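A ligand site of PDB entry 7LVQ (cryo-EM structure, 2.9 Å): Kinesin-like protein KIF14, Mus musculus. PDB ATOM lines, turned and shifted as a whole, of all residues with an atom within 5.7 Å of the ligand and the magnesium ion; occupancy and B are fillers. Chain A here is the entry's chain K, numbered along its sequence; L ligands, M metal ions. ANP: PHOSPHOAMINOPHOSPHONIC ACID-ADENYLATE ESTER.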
ATOM      1  N   ARG A  14      18.547 -10.026   6.473  1.00  0.00           N
ATOM      2  CA  ARG A  14      17.185 -10.474   6.154  1.00  0.00           C
ATOM      3  C   ARG A  14      16.144  -9.760   7.020  1.00  0.00           C
ATOM      4  O   ARG A  14      16.438  -9.518   8.200  1.00  0.00           O
ATOM      5  CB  ARG A  14      17.123 -11.988   6.344  1.00  0.00           C
ATOM      6  CG  ARG A  14      15.771 -12.619   6.080  1.00  0.00           C
ATOM      7  CD  ARG A  14      15.959 -14.109   6.173  1.00  0.00           C
ATOM      8  NE  ARG A  14      15.225 -14.819   5.157  1.00  0.00           N
ATOM      9  CZ  ARG A  14      15.301 -16.135   4.974  1.00  0.00           C
ATOM     10  NH1 ARG A  14      16.157 -16.844   5.696  1.00  0.00           N
ATOM     11  NH2 ARG A  14      14.541 -16.723   4.073  1.00  0.00           N
ATOM     12  N   VAL A  15      14.976  -9.475   6.456  1.00  0.00           N
ATOM     13  CA  VAL A  15      13.864  -8.822   7.122  1.00  0.00           C
ATOM     14  C   VAL A  15      12.744  -9.837   7.298  1.00  0.00           C
ATOM     15  O   VAL A  15      12.045 -10.172   6.333  1.00  0.00           O
ATOM     16  CB  VAL A  15      13.369  -7.610   6.348  1.00  0.00           C
ATOM     17  CG1 VAL A  15      12.249  -6.955   7.085  1.00  0.00           C
ATOM     18  CG2 VAL A  15      14.462  -6.620   6.098  1.00  0.00           C
ATOM     19  N   ARG A  16      12.532 -10.368   8.491  1.00  0.00           N
ATOM     20  CA  ARG A  16      11.505 -11.420   8.737  1.00  0.00           C
ATOM     21  C   ARG A  16      10.109 -10.797   8.683  1.00  0.00           C
ATOM     22  O   ARG A  16      10.003  -9.604   8.915  1.00  0.00           O
ATOM     23  CB  ARG A  16      11.846 -12.095  10.083  1.00  0.00           C
ATOM     24  CG  ARG A  16      10.671 -12.635  10.888  1.00  0.00           C
ATOM     25  CD  ARG A  16      10.935 -12.941  12.335  1.00  0.00           C
ATOM     26  NE  ARG A  16      10.833 -11.751  13.153  1.00  0.00           N
ATOM     27  CZ  ARG A  16       9.737 -11.363  13.771  1.00  0.00           C
ATOM     28  NH1 ARG A  16       8.561 -11.731  13.309  1.00  0.00           N
ATOM     29  NH2 ARG A  16       9.828 -10.663  14.884  1.00  0.00           N
ATOM     30  N   PRO A  17       9.042 -11.555   8.331  1.00  0.00           N
ATOM     31  CA  PRO A  17       7.679 -11.024   8.391  1.00  0.00           C
ATOM     32  C   PRO A  17       7.147 -10.837   9.822  1.00  0.00           C
ATOM     33  O   PRO A  17       7.750 -11.294  10.768  1.00  0.00           O
ATOM     34  CB  PRO A  17       6.838 -12.025   7.583  1.00  0.00           C
ATOM     35  CG  PRO A  17       7.564 -13.307   7.789  1.00  0.00           C
ATOM     36  CD  PRO A  17       9.007 -12.880   7.721  1.00  0.00           C
ATOM     37  N   SER A  59      11.653 -11.167   3.122  1.00  0.00           N
ATOM     38  CA  SER A  59      10.591 -12.203   3.242  1.00  0.00           C
ATOM     39  C   SER A  59       9.422 -11.593   4.009  1.00  0.00           C
ATOM     40  O   SER A  59       8.629 -12.370   4.577  1.00  0.00           O
ATOM     41  CB  SER A  59      11.139 -13.436   3.909  1.00  0.00           C
ATOM     42  OG  SER A  59      10.090 -14.297   4.326  1.00  0.00           O
ATOM     43  N   GLN A  98      18.034 -10.792  17.362  1.00  0.00           N
ATOM     44  CA  GLN A  98      17.447 -10.673  18.723  1.00  0.00           C
ATOM     45  C   GLN A  98      16.378 -11.748  18.915  1.00  0.00           C
ATOM     46  O   GLN A  98      16.108 -12.478  17.959  1.00  0.00           O
ATOM     47  CB  GLN A  98      16.853  -9.292  18.923  1.00  0.00           C
ATOM     48  CG  GLN A  98      15.571  -9.084  18.154  1.00  0.00           C
ATOM     49  CD  GLN A  98      15.036  -7.689  18.339  1.00  0.00           C
ATOM     50  OE1 GLN A  98      15.323  -6.787  17.553  1.00  0.00           O
ATOM     51  NE2 GLN A  98      14.286  -7.493  19.414  1.00  0.00           N
ATOM     52  N   THR A  99      15.709 -11.804  20.057  1.00  0.00           N
ATOM     53  CA  THR A  99      14.728 -12.881  20.310  1.00  0.00           C
ATOM     54  C   THR A  99      13.614 -12.818  19.259  1.00  0.00           C
ATOM     55  O   THR A  99      13.155 -11.707  18.977  1.00  0.00           O
ATOM     56  CB  THR A  99      14.185 -12.762  21.741  1.00  0.00           C
ATOM     57  OG1 THR A  99      15.252 -12.357  22.595  1.00  0.00           O
ATOM     58  CG2 THR A  99      13.590 -14.050  22.256  1.00  0.00           C
ATOM     59  N   GLY A 100      13.204 -13.944  18.695  1.00  0.00           N
ATOM     60  CA  GLY A 100      12.129 -14.021  17.696  1.00  0.00           C
ATOM     61  C   GLY A 100      12.531 -13.451  16.348  1.00  0.00           C
ATOM     62  O   GLY A 100      11.614 -13.295  15.527  1.00  0.00           O
ATOM     63  N   SER A 101      13.800 -13.209  16.049  1.00  0.00           N
ATOM     64  CA  SER A 101      14.155 -12.532  14.771  1.00  0.00           C
ATOM     65  C   SER A 101      14.437 -13.478  13.606  1.00  0.00           C
ATOM     66  O   SER A 101      14.613 -12.941  12.508  1.00  0.00           O
ATOM     67  CB  SER A 101      15.300 -11.606  14.964  1.00  0.00           C
ATOM     68  OG  SER A 101      16.427 -12.306  15.442  1.00  0.00           O
ATOM     69  N   GLY A 102      14.415 -14.801  13.746  1.00  0.00           N
ATOM     70  CA  GLY A 102      14.618 -15.659  12.562  1.00  0.00           C
ATOM     71  C   GLY A 102      16.014 -16.219  12.371  1.00  0.00           C
ATOM     72  O   GLY A 102      16.231 -16.787  11.295  1.00  0.00           O
ATOM     73  N   LYS A 103      16.948 -16.097  13.294  1.00  0.00           N
ATOM     74  CA  LYS A 103      18.267 -16.727  13.074  1.00  0.00           C
ATOM     75  C   LYS A 103      18.105 -18.245  12.974  1.00  0.00           C
ATOM     76  O   LYS A 103      18.691 -18.829  12.045  1.00  0.00           O
ATOM     77  CB  LYS A 103      19.214 -16.424  14.236  1.00  0.00           C
ATOM     78  CG  LYS A 103      19.411 -14.951  14.550  1.00  0.00           C
ATOM     79  CD  LYS A 103      19.756 -14.744  15.993  1.00  0.00           C
ATOM     80  CE  LYS A 103      18.658 -15.248  16.893  1.00  0.00           C
ATOM     81  NZ  LYS A 103      18.754 -14.634  18.236  1.00  0.00           N
ATOM     82  N   SER A 104      17.348 -18.862  13.863  1.00  0.00           N
ATOM     83  CA  SER A 104      17.107 -20.332  13.851  1.00  0.00           C
ATOM     84  C   SER A 104      16.398 -20.744  12.558  1.00  0.00           C
ATOM     85  O   SER A 104      16.781 -21.778  12.001  1.00  0.00           O
ATOM     86  CB  SER A 104      16.295 -20.728  15.041  1.00  0.00           C
ATOM     87  OG  SER A 104      16.990 -20.431  16.249  1.00  0.00           O
ATOM     88  N   TYR A 105      15.435 -19.988  12.100  1.00  0.00           N
ATOM     89  CA  TYR A 105      14.694 -20.324  10.851  1.00  0.00           C
ATOM     90  C   TYR A 105      15.619 -20.233   9.641  1.00  0.00           C
ATOM     91  O   TYR A 105      15.512 -21.087   8.752  1.00  0.00           O
ATOM     92  CB  TYR A 105      13.487 -19.399  10.671  1.00  0.00           C
ATOM     93  CG  TYR A 105      12.955 -19.331   9.267  1.00  0.00           C
ATOM     94  CD1 TYR A 105      11.837 -20.057   8.894  1.00  0.00           C
ATOM     95  CD2 TYR A 105      13.556 -18.538   8.310  1.00  0.00           C
ATOM     96  CE1 TYR A 105      11.334 -19.999   7.601  1.00  0.00           C
ATOM     97  CE2 TYR A 105      13.073 -18.459   7.019  1.00  0.00           C
ATOM     98  CZ  TYR A 105      11.960 -19.192   6.661  1.00  0.00           C
ATOM     99  OH  TYR A 105      11.475 -19.113   5.384  1.00  0.00           O
ATOM    100  N   THR A 106      16.529 -19.266   9.611  1.00  0.00           N
ATOM    101  CA  THR A 106      17.416 -19.034   8.442  1.00  0.00           C
ATOM    102  C   THR A 106      18.551 -20.043   8.373  1.00  0.00           C
ATOM    103  O   THR A 106      18.941 -20.410   7.264  1.00  0.00           O
ATOM    104  CB  THR A 106      18.044 -17.636   8.499  1.00  0.00           C
ATOM    105  OG1 THR A 106      17.050 -16.687   8.096  1.00  0.00           O
ATOM    106  CG2 THR A 106      19.264 -17.507   7.625  1.00  0.00           C
ATOM    107  N   LEU A 110      12.769 -25.539   9.847  1.00  0.00           N
ATOM    108  CA  LEU A 110      11.678 -26.363  10.407  1.00  0.00           C
ATOM    109  C   LEU A 110      11.648 -27.690   9.662  1.00  0.00           C
ATOM    110  O   LEU A 110      12.437 -27.897   8.721  1.00  0.00           O
ATOM    111  CB  LEU A 110      10.391 -25.548  10.227  1.00  0.00           C
ATOM    112  CG  LEU A 110      10.477 -24.074  10.625  1.00  0.00           C
ATOM    113  CD1 LEU A 110       9.241 -23.322  10.182  1.00  0.00           C
ATOM    114  CD2 LEU A 110      10.674 -23.937  12.130  1.00  0.00           C
ATOM    115  N   ARG A 206      19.437 -29.102  22.527  1.00  0.00           N
ATOM    116  CA  ARG A 206      19.748 -27.694  22.692  1.00  0.00           C
ATOM    117  C   ARG A 206      18.804 -27.048  23.687  1.00  0.00           C
ATOM    118  O   ARG A 206      17.604 -27.361  23.720  1.00  0.00           O
ATOM    119  CB  ARG A 206      19.651 -26.970  21.355  1.00  0.00           C
ATOM    120  CG  ARG A 206      20.352 -25.683  21.332  1.00  0.00           C
ATOM    121  CD  ARG A 206      20.304 -25.065  20.004  1.00  0.00           C
ATOM    122  NE  ARG A 206      20.655 -23.665  20.046  1.00  0.00           N
ATOM    123  CZ  ARG A 206      20.682 -22.870  18.994  1.00  0.00           C
ATOM    124  NH1 ARG A 206      20.389 -23.317  17.785  1.00  0.00           N
ATOM    125  NH2 ARG A 206      21.016 -21.601  19.138  1.00  0.00           N
ATOM    126  N   ASN A 214       8.989 -15.503  21.768  1.00  0.00           N
ATOM    127  CA  ASN A 214       8.719 -16.792  21.084  1.00  0.00           C
ATOM    128  C   ASN A 214       8.721 -17.848  22.212  1.00  0.00           C
ATOM    129  O   ASN A 214       9.593 -17.740  23.084  1.00  0.00           O
ATOM    130  CB  ASN A 214       9.724 -17.093  19.974  1.00  0.00           C
ATOM    131  CG  ASN A 214      11.144 -16.747  20.361  1.00  0.00           C
ATOM    132  OD1 ASN A 214      11.367 -16.231  21.452  1.00  0.00           O
ATOM    133  ND2 ASN A 214      12.087 -17.030  19.484  1.00  0.00           N
ATOM    134  N   LYS A 216       9.446 -20.992  21.927  1.00  0.00           N
ATOM    135  CA  LYS A 216      10.535 -21.949  21.672  1.00  0.00           C
ATOM    136  C   LYS A 216      11.790 -21.125  21.412  1.00  0.00           C
ATOM    137  O   LYS A 216      12.381 -21.255  20.322  1.00  0.00           O
ATOM    138  CB  LYS A 216      10.185 -22.866  20.490  1.00  0.00           C
ATOM    139  CG  LYS A 216      11.157 -24.009  20.268  1.00  0.00           C
ATOM    140  CD  LYS A 216      10.508 -25.272  19.741  1.00  0.00           C
ATOM    141  CE  LYS A 216      11.445 -26.465  19.787  1.00  0.00           C
ATOM    142  NZ  LYS A 216      11.918 -26.741  21.168  1.00  0.00           N
ATOM    143  N   SER A 217      12.171 -20.308  22.394  1.00  0.00           N
ATOM    144  CA  SER A 217      13.326 -19.385  22.318  1.00  0.00           C
ATOM    145  C   SER A 217      14.636 -20.158  22.429  1.00  0.00           C
ATOM    146  O   SER A 217      14.617 -21.273  22.956  1.00  0.00           O
ATOM    147  CB  SER A 217      13.239 -18.330  23.369  1.00  0.00           C
ATOM    148  OG  SER A 217      14.482 -17.660  23.489  1.00  0.00           O
ATOM    149  N   SER A 218      15.720 -19.590  21.932  1.00  0.00           N
ATOM    150  CA  SER A 218      17.052 -20.238  21.971  1.00  0.00           C
ATOM    151  C   SER A 218      17.860 -19.632  23.129  1.00  0.00           C
ATOM    152  O   SER A 218      18.112 -18.421  23.064  1.00  0.00           O
ATOM    153  CB  SER A 218      17.753 -20.088  20.667  1.00  0.00           C
ATOM    154  OG  SER A 218      17.161 -20.920  19.686  1.00  0.00           O
ATOM    155  N   ASP A 253      24.688 -20.384  15.048  1.00  0.00           N
ATOM    156  CA  ASP A 253      23.384 -19.843  15.429  1.00  0.00           C
ATOM    157  C   ASP A 253      23.445 -19.352  16.864  1.00  0.00           C
ATOM    158  O   ASP A 253      23.586 -20.139  17.795  1.00  0.00           O
ATOM    159  CB  ASP A 253      22.296 -20.877  15.282  1.00  0.00           C
ATOM    160  CG  ASP A 253      20.984 -20.426  15.864  1.00  0.00           C
ATOM    161  OD1 ASP A 253      20.677 -19.215  15.777  1.00  0.00           O
ATOM    162  OD2 ASP A 253      20.268 -21.268  16.437  1.00  0.00           O
ATOM    163  N   LEU A 254      23.359 -18.010  17.088  1.00  0.00           N
ATOM    164  CA  LEU A 254      23.498 -17.367  18.429  1.00  0.00           C
ATOM    165  C   LEU A 254      22.117 -17.163  19.087  1.00  0.00           C
ATOM    166  O   LEU A 254      21.116 -17.483  18.432  1.00  0.00           O
ATOM    167  CB  LEU A 254      24.185 -16.004  18.252  1.00  0.00           C
ATOM    168  CG  LEU A 254      25.554 -15.961  17.599  1.00  0.00           C
ATOM    169  CD1 LEU A 254      26.094 -14.544  17.623  1.00  0.00           C
ATOM    170  CD2 LEU A 254      26.536 -16.859  18.306  1.00  0.00           C
ATOM    171  N   ALA A 255      22.075 -16.651  20.323  1.00  0.00           N
ATOM    172  CA  ALA A 255      20.833 -16.345  21.089  1.00  0.00           C
ATOM    173  C   ALA A 255      20.529 -14.842  21.009  1.00  0.00           C
ATOM    174  O   ALA A 255      21.331 -14.119  20.408  1.00  0.00           O
ATOM    175  CB  ALA A 255      21.006 -16.836  22.501  1.00  0.00           C
ATOM    176  N   GLY A 256      19.424 -14.354  21.588  1.00  0.00           N
ATOM    177  CA  GLY A 256      19.023 -12.924  21.491  1.00  0.00           C
ATOM    178  C   GLY A 256      19.448 -12.059  22.670  1.00  0.00           C
ATOM    179  O   GLY A 256      19.755 -12.614  23.723  1.00  0.00           O
ATOM    180  N   GLU A 258      17.703 -10.017  24.658  1.00  0.00           N
ATOM    181  CA  GLU A 258      16.897 -10.338  25.833  1.00  0.00           C
ATOM    182  C   GLU A 258      16.848  -9.195  26.829  1.00  0.00           C
ATOM    183  O   GLU A 258      17.402  -9.245  27.929  1.00  0.00           O
ATOM    184  CB  GLU A 258      17.401 -11.617  26.489  1.00  0.00           C
ATOM    185  CG  GLU A 258      16.358 -12.323  27.301  1.00  0.00           C
ATOM    186  CD  GLU A 258      15.480 -13.237  26.464  1.00  0.00           C
ATOM    187  OE1 GLU A 258      16.039 -14.078  25.717  1.00  0.00           O
ATOM    188  OE2 GLU A 258      14.242 -13.123  26.537  1.00  0.00           O
HETATM  189  PG  ANP L   1      16.111 -16.823  19.368  1.00  0.00           P
HETATM  190  O1G ANP L   1      17.476 -17.321  19.044  1.00  0.00           O
HETATM  191  O2G ANP L   1      15.063 -17.854  19.611  1.00  0.00           O
HETATM  192  O3G ANP L   1      16.119 -15.770  20.425  1.00  0.00           O
HETATM  193  PB  ANP L   1      15.202 -17.207  16.630  1.00  0.00           P
HETATM  194  O1B ANP L   1      16.220 -16.937  15.591  1.00  0.00           O
HETATM  195  O2B ANP L   1      15.115 -18.604  17.178  1.00  0.00           O
HETATM  196  N3B ANP L   1      15.688 -16.112  17.868  1.00  0.00           N
HETATM  197  PA  ANP L   1      12.960 -18.171  15.555  1.00  0.00           P
HETATM  198  O1A ANP L   1      13.679 -18.836  14.439  1.00  0.00           O
HETATM  199  O2A ANP L   1      12.624 -18.951  16.788  1.00  0.00           O
HETATM  200  O3A ANP L   1      13.795 -16.891  15.984  1.00  0.00           O
HETATM  201  O5' ANP L   1      11.626 -17.544  14.946  1.00  0.00           O
HETATM  202  C5' ANP L   1      10.393 -17.778  15.607  1.00  0.00           C
HETATM  203  C4' ANP L   1       9.363 -18.149  14.550  1.00  0.00           C
HETATM  204  O4' ANP L   1       9.428 -17.249  13.457  1.00  0.00           O
HETATM  205  C3' ANP L   1       9.626 -19.533  14.008  1.00  0.00           C
HETATM  206  O3' ANP L   1       8.674 -20.449  14.545  1.00  0.00           O
HETATM  207  C2' ANP L   1       9.527 -19.399  12.501  1.00  0.00           C
HETATM  208  O2' ANP L   1       8.549 -20.272  11.929  1.00  0.00           O
HETATM  209  C1' ANP L   1       9.116 -17.968  12.288  1.00  0.00           C
HETATM  210  N9  ANP L   1       9.897 -17.368  11.224  1.00  0.00           N
HETATM  211  C8  ANP L   1      11.165 -17.011  11.391  1.00  0.00           C
HETATM  212  N7  ANP L   1      11.645 -16.487  10.248  1.00  0.00           N
HETATM  213  C5  ANP L   1      10.662 -16.543   9.331  1.00  0.00           C
HETATM  214  C6  ANP L   1      10.519 -16.180   7.912  1.00  0.00           C
HETATM  215  N6  ANP L   1      11.536 -15.609   7.236  1.00  0.00           N
HETATM  216  N1  ANP L   1       9.325 -16.382   7.344  1.00  0.00           N
HETATM  217  C2  ANP L   1       8.296 -16.940   8.004  1.00  0.00           C
HETATM  218  N3  ANP L   1       8.373 -17.305   9.286  1.00  0.00           N
HETATM  219  C4  ANP L   1       9.502 -17.133   9.990  1.00  0.00           C
HETATM  220 MG    MG M   1      16.984 -19.313  18.172  1.00  0.00          MG
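N of Tyr 105 lies within hydrogen-bond range of O1A of the ligand, at 3.1 Å. N of Lys 103 sits at hydrogen-bond distance from O1B of the ligand (2.6 Å). O2G of the ligand is in hydrogen-bond range of N of Ser 218 (3.0 Å). An oxygen (O3G) of the ligand lies within salt-bridge range of the side-chain amino group (NZ) of Lys 103. N of Ser 104 sits at hydrogen-bond distance from O1B of the ligand, 2.8 Å away. O2G of the ligand lies within hydrogen-bond range of ND2 of Asn 214 (3.1 Å). O3A of the ligand lies within hydrogen-bond range of N of Gly 102 (3.1 Å).
NZ of Lys 103 lies within hydrogen-bond range of O of Gln 98 (3.4 Å). The side-chain amide nitrogen (ND2) of Asn 214 lies close to the backbone NH (N) of Gly 100 (3.4 Å). OG of Ser 101 sits at hydrogen-bond distance from O of Gln 98 (2.5 Å). The backbone carbonyl oxygen (O) of Gly 100 sits at hydrogen-bond distance from the guanidinium group (NE) of Arg 16, 2.9 Å away. O of Gly 102 sits at hydrogen-bond distance from OG1 of Thr 106, at 3.3 Å. N of Ser 59 is in hydrogen-bond range of O of Val 15. O of Ala 255 sits close to NZ of Lys 103 (3.4 Å). The side-chain hydroxyl (OG) of Ser 104 sits close to the side-chain carboxylate (OD2) of Asp 253 (3.4 Å).
N of Gly 100 lies close to N3B of the ligand, 3.4 Å away. Pro 17 touches the ligand (CD to N1, 3.5 Å). Ser 59 touches the ligand. Gln 98 touches the ligand (O to N3B, 3.7 Å). Thr 99 touches the ligand. Ser 101 touches the ligand (N to O3A, 3.7 Å). CD1 of Leu 110 touches O2' of the ligand, 3.6 Å away. CA of Ser 217 touches O2G of the ligand, at 3.6 Å. Leu 254 touches the ligand. Gly 256 touches the ligand. Of the 25 residues printed, 16 come within 4 Å of the ligand. The nearest printed residue that does not touch the ligand is Arg 16 (4.02 Å).
Of the 25 residues printed, 2 come within 4 Å of the magnesium ion.
The side-chain hydroxyl (OG) of Ser 218 is bound to the magnesium ion (2.2 Å). The magnesium ion is bound by the side-chain hydroxyl (OG) of Ser 104 (2.2 Å). An oxygen (O1G) of the ligand is bound to the magnesium ion (2.2 Å). O2B of the ligand binds the magnesium ion (2.2 Å). The magnesium ion has four donor atoms within binding distance. Slightly farther from the magnesium ion lies O2G of the ligand (2.8 Å).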
